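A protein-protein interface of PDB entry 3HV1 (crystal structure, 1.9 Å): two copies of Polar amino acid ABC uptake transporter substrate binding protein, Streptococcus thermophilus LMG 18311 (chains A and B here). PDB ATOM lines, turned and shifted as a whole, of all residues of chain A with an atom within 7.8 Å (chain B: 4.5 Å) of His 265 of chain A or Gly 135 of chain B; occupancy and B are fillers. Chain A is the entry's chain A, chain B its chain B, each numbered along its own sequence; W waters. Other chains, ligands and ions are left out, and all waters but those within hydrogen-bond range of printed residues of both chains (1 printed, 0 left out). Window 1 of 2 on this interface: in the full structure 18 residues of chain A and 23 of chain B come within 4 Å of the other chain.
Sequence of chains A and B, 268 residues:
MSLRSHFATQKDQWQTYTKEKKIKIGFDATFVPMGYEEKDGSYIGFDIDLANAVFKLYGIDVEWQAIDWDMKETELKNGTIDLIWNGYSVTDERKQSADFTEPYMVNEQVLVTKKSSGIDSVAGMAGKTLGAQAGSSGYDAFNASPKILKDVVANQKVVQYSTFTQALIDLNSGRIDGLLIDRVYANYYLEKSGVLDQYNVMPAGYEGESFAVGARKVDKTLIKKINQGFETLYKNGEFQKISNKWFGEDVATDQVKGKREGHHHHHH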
ATOM      1  N   VAL A  90     -23.147  -8.922  33.656  1.00  0.00           N
ATOM      2  CA  VAL A  90     -23.836 -10.201  33.545  1.00  0.00           C
ATOM      3  C   VAL A  90     -23.098 -11.358  34.210  1.00  0.00           C
ATOM      4  O   VAL A  90     -21.869 -11.437  34.172  1.00  0.00           O
ATOM      5  CB  VAL A  90     -24.076 -10.579  32.057  1.00  0.00           C
ATOM      6  CG1 VAL A  90     -24.753 -11.945  31.955  1.00  0.00           C
ATOM      7  CG2 VAL A  90     -24.934  -9.523  31.386  1.00  0.00           C
ATOM      8  N   LYS A  95     -28.471 -13.318  36.088  1.00  0.00           N
ATOM      9  CA  LYS A  95     -29.447 -13.534  35.032  1.00  0.00           C
ATOM     10  C   LYS A  95     -30.689 -14.235  35.572  1.00  0.00           C
ATOM     11  O   LYS A  95     -31.755 -14.180  34.965  1.00  0.00           O
ATOM     12  CB  LYS A  95     -28.828 -14.352  33.901  1.00  0.00           C
ATOM     13  CG  LYS A  95     -27.752 -13.605  33.133  1.00  0.00           C
ATOM     14  CD  LYS A  95     -27.220 -14.426  31.970  1.00  0.00           C
ATOM     15  CE  LYS A  95     -28.293 -14.663  30.926  1.00  0.00           C
ATOM     16  NZ  LYS A  95     -27.739 -15.337  29.720  1.00  0.00           N
ATOM     17  N   GLU A 102     -27.341  -4.226  26.508  1.00  0.00           N
ATOM     18  CA  GLU A 102     -26.092  -4.570  25.847  1.00  0.00           C
ATOM     19  C   GLU A 102     -25.016  -3.894  26.698  1.00  0.00           C
ATOM     20  O   GLU A 102     -25.317  -2.971  27.456  1.00  0.00           O
ATOM     21  CB  GLU A 102     -26.073  -3.980  24.434  1.00  0.00           C
ATOM     22  CG  GLU A 102     -27.104  -4.582  23.509  1.00  0.00           C
ATOM     23  CD  GLU A 102     -26.996  -6.088  23.448  1.00  0.00           C
ATOM     24  OE1 GLU A 102     -25.858  -6.586  23.299  1.00  0.00           O
ATOM     25  OE2 GLU A 102     -28.042  -6.775  23.546  1.00  0.00           O
ATOM     26  N   GLY A 262     -21.696 -10.254  14.412  1.00  0.00           N
ATOM     27  CA  GLY A 262     -21.062 -11.255  15.252  1.00  0.00           C
ATOM     28  C   GLY A 262     -21.621 -11.394  16.654  1.00  0.00           C
ATOM     29  O   GLY A 262     -21.097 -12.166  17.453  1.00  0.00           O
ATOM     30  N   HIS A 263     -22.686 -10.666  16.964  1.00  0.00           N
ATOM     31  CA  HIS A 263     -23.262 -10.740  18.300  1.00  0.00           C
ATOM     32  C   HIS A 263     -24.590 -11.489  18.379  1.00  0.00           C
ATOM     33  O   HIS A 263     -25.209 -11.553  19.441  1.00  0.00           O
ATOM     34  CB  HIS A 263     -23.408  -9.330  18.880  1.00  0.00           C
ATOM     35  CG  HIS A 263     -22.097  -8.669  19.176  1.00  0.00           C
ATOM     36  ND1 HIS A 263     -21.240  -9.128  20.155  1.00  0.00           N
ATOM     37  CD2 HIS A 263     -21.481  -7.607  18.604  1.00  0.00           C
ATOM     38  CE1 HIS A 263     -20.152  -8.377  20.171  1.00  0.00           C
ATOM     39  NE2 HIS A 263     -20.273  -7.448  19.240  1.00  0.00           N
ATOM     40  N   HIS A 264     -25.021 -12.062  17.258  1.00  0.00           N
ATOM     41  CA  HIS A 264     -26.266 -12.821  17.238  1.00  0.00           C
ATOM     42  C   HIS A 264     -26.016 -14.223  17.814  1.00  0.00           C
ATOM     43  O   HIS A 264     -25.051 -14.891  17.440  1.00  0.00           O
ATOM     44  CB  HIS A 264     -26.806 -12.944  15.806  1.00  0.00           C
ATOM     45  CG  HIS A 264     -26.997 -11.632  15.108  1.00  0.00           C
ATOM     46  ND1 HIS A 264     -25.943 -10.881  14.632  1.00  0.00           N
ATOM     47  CD2 HIS A 264     -28.119 -10.935  14.811  1.00  0.00           C
ATOM     48  CE1 HIS A 264     -26.407  -9.779  14.072  1.00  0.00           C
ATOM     49  NE2 HIS A 264     -27.725  -9.786  14.167  1.00  0.00           N
ATOM     50  N   HIS A 265     -26.883 -14.642  18.734  1.00  0.00           N
ATOM     51  CA  HIS A 265     -26.808 -15.954  19.388  1.00  0.00           C
ATOM     52  C   HIS A 265     -28.103 -16.700  19.082  1.00  0.00           C
ATOM     53  O   HIS A 265     -29.183 -16.216  19.420  1.00  0.00           O
ATOM     54  CB  HIS A 265     -26.664 -15.790  20.905  1.00  0.00           C
ATOM     55  CG  HIS A 265     -27.546 -14.727  21.483  1.00  0.00           C
ATOM     56  ND1 HIS A 265     -28.837 -14.513  21.050  1.00  0.00           N
ATOM     57  CD2 HIS A 265     -27.323 -13.816  22.460  1.00  0.00           C
ATOM     58  CE1 HIS A 265     -29.369 -13.514  21.731  1.00  0.00           C
ATOM     59  NE2 HIS A 265     -28.472 -13.074  22.594  1.00  0.00           N
ATOM     60  N   HIS A 266     -27.988 -17.878  18.465  1.00  0.00           N
ATOM     61  CA  HIS A 266     -29.147 -18.684  18.060  1.00  0.00           C
ATOM     62  C   HIS A 266     -30.469 -17.968  18.339  1.00  0.00           C
ATOM     63  O   HIS A 266     -31.275 -18.392  19.172  1.00  0.00           O
ATOM     64  CB  HIS A 266     -29.095 -20.085  18.702  1.00  0.00           C
ATOM     65  CG  HIS A 266     -29.456 -20.128  20.155  1.00  0.00           C
ATOM     66  ND1 HIS A 266     -28.865 -19.318  21.102  1.00  0.00           N
ATOM     67  CD2 HIS A 266     -30.319 -20.926  20.828  1.00  0.00           C
ATOM     68  CE1 HIS A 266     -29.349 -19.616  22.296  1.00  0.00           C
ATOM     69  NE2 HIS A 266     -30.233 -20.589  22.157  1.00  0.00           N
ATOM     70  N   HIS A 267     -30.666 -16.868  17.607  1.00  0.00           N
ATOM     71  CA  HIS A 267     -31.840 -16.017  17.747  1.00  0.00           C
ATOM     72  C   HIS A 267     -33.087 -16.585  17.089  1.00  0.00           C
ATOM     73  O   HIS A 267     -33.883 -15.775  16.561  1.00  0.00           O
ATOM     74  CB  HIS A 267     -31.544 -14.615  17.182  1.00  0.00           C
ATOM     75  CG  HIS A 267     -31.446 -14.551  15.682  1.00  0.00           C
ATOM     76  ND1 HIS A 267     -31.264 -13.363  15.004  1.00  0.00           N
ATOM     77  CD2 HIS A 267     -31.563 -15.509  14.731  1.00  0.00           C
ATOM     78  CE1 HIS A 267     -31.283 -13.590  13.703  1.00  0.00           C
ATOM     79  NE2 HIS A 267     -31.464 -14.885  13.511  1.00  0.00           N
ATOM     80  N   GLN B 133     -17.179 -16.891  23.221  1.00  0.00           N
ATOM     81  CA  GLN B 133     -17.791 -15.578  23.087  1.00  0.00           C
ATOM     82  C   GLN B 133     -18.721 -15.252  24.256  1.00  0.00           C
ATOM     83  O   GLN B 133     -19.586 -16.044  24.612  1.00  0.00           O
ATOM     84  CB  GLN B 133     -18.565 -15.514  21.766  1.00  0.00           C
ATOM     85  CG  GLN B 133     -19.431 -14.284  21.596  1.00  0.00           C
ATOM     86  CD  GLN B 133     -20.059 -14.204  20.219  1.00  0.00           C
ATOM     87  OE1 GLN B 133     -20.727 -15.136  19.771  1.00  0.00           O
ATOM     88  NE2 GLN B 133     -19.847 -13.083  19.539  1.00  0.00           N
ATOM     89  N   ALA B 134     -18.535 -14.080  24.849  1.00  0.00           N
ATOM     90  CA  ALA B 134     -19.374 -13.658  25.963  1.00  0.00           C
ATOM     91  C   ALA B 134     -20.852 -13.705  25.571  1.00  0.00           C
ATOM     92  O   ALA B 134     -21.230 -13.266  24.484  1.00  0.00           O
ATOM     93  CB  ALA B 134     -18.995 -12.250  26.391  1.00  0.00           C
ATOM     94  N   GLY B 135     -21.675 -14.254  26.460  1.00  0.00           N
ATOM     95  CA  GLY B 135     -23.106 -14.345  26.220  1.00  0.00           C
ATOM     96  C   GLY B 135     -23.548 -15.084  24.972  1.00  0.00           C
ATOM     97  O   GLY B 135     -24.650 -14.858  24.473  1.00  0.00           O
ATOM     98  N   SER B 136     -22.702 -15.973  24.463  1.00  0.00           N
ATOM     99  CA  SER B 136     -23.043 -16.734  23.265  1.00  0.00           C
ATOM    100  C   SER B 136     -23.683 -18.054  23.662  1.00  0.00           C
ATOM    101  O   SER B 136     -23.602 -18.463  24.820  1.00  0.00           O
ATOM    102  CB  SER B 136     -21.783 -17.015  22.442  1.00  0.00           C
ATOM    103  OG  SER B 136     -20.904 -17.860  23.167  1.00  0.00           O
ATOM    104  N   SER B 137     -24.319 -18.718  22.701  1.00  0.00           N
ATOM    105  CA  SER B 137     -24.949 -20.003  22.964  1.00  0.00           C
ATOM    106  C   SER B 137     -23.862 -21.022  23.309  1.00  0.00           C
ATOM    107  O   SER B 137     -24.116 -22.016  23.995  1.00  0.00           O
ATOM    108  CB  SER B 137     -25.756 -20.466  21.742  1.00  0.00           C
ATOM    109  OG  SER B 137     -24.982 -20.427  20.558  1.00  0.00           O
ATOM    110  N   GLN B 160     -13.784 -15.615  28.264  1.00  0.00           N
ATOM    111  CA  GLN B 160     -14.769 -14.954  27.420  1.00  0.00           C
ATOM    112  C   GLN B 160     -14.215 -13.768  26.644  1.00  0.00           C
ATOM    113  O   GLN B 160     -13.447 -12.968  27.173  1.00  0.00           O
ATOM    114  CB  GLN B 160     -15.968 -14.520  28.265  1.00  0.00           C
ATOM    115  CG  GLN B 160     -16.692 -15.690  28.902  1.00  0.00           C
ATOM    116  CD  GLN B 160     -17.965 -15.284  29.605  1.00  0.00           C
ATOM    117  OE1 GLN B 160     -18.930 -14.856  28.973  1.00  0.00           O
ATOM    118  NE2 GLN B 160     -17.974 -15.419  30.926  1.00  0.00           N
HETATM  119  O   HOH W   1     -23.291 -14.891  19.756  1.00  0.00           O
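O of Gly 262 of chain A is in hydrogen-bond range of NE2 of Gln 133 of chain B (2.6 Å).
The backbone carbonyl oxygen (O) of Gln 133 of chain B lies within hydrogen-bond range of the side-chain hydroxyl (OG) of Ser 136 of chain B (2.7 Å).
Among the printed residues, merely in contact across the chains: His 266 of chain A with Ser 137 of chain B (3.4 Å) and His 265 of chain A with Gly 135 of chain B (3.5 Å).
Of chain A, only His 265 comes within 4 Å of Gly 135 of chain B.
Printed residues of chain A within 4 Å of Gln 133 of chain B: Gly 262 (2.6 Å).
Of the printed residues of chain A, Ser 137 of chain B touches His 266 (3.4 Å).
Val 90 of chain A touches none of the printed residues of chain B.
The nearest residue of chain A that does not touch Gly 135 of chain B is Lys 95 of chain A (5.9 Å).
The nearest printed residue of chain A that does not touch Gln 133 of chain B is His 263 of chain A (4.2 Å).
Printed residues of chain B that touch a printed residue of chain A: Gln 133, Gly 135 and Ser 137.
Of the 9 printed residues of chain A, 3 touch a printed residue of chain B.
Printed residues of chain A that touch a printed residue of chain B: Gly 262, His 265 and His 266.
Hydrophobic or aromatic side chains of chain A within 4 Å of the printed part of chain B: His 265 and His 266.
Among the printed residues, 3 pairs touch across the chains.
Among the printed residues, no Asp or Glu carboxylate lies within 4 Å of a Lys or Arg side-chain nitrogen of the other chain.
No position is printed for both chains.
Water W1 bridges OE1 of Gln 133 of chain B (2.6 Å) and O of His 264 of chain A (2.9 Å).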
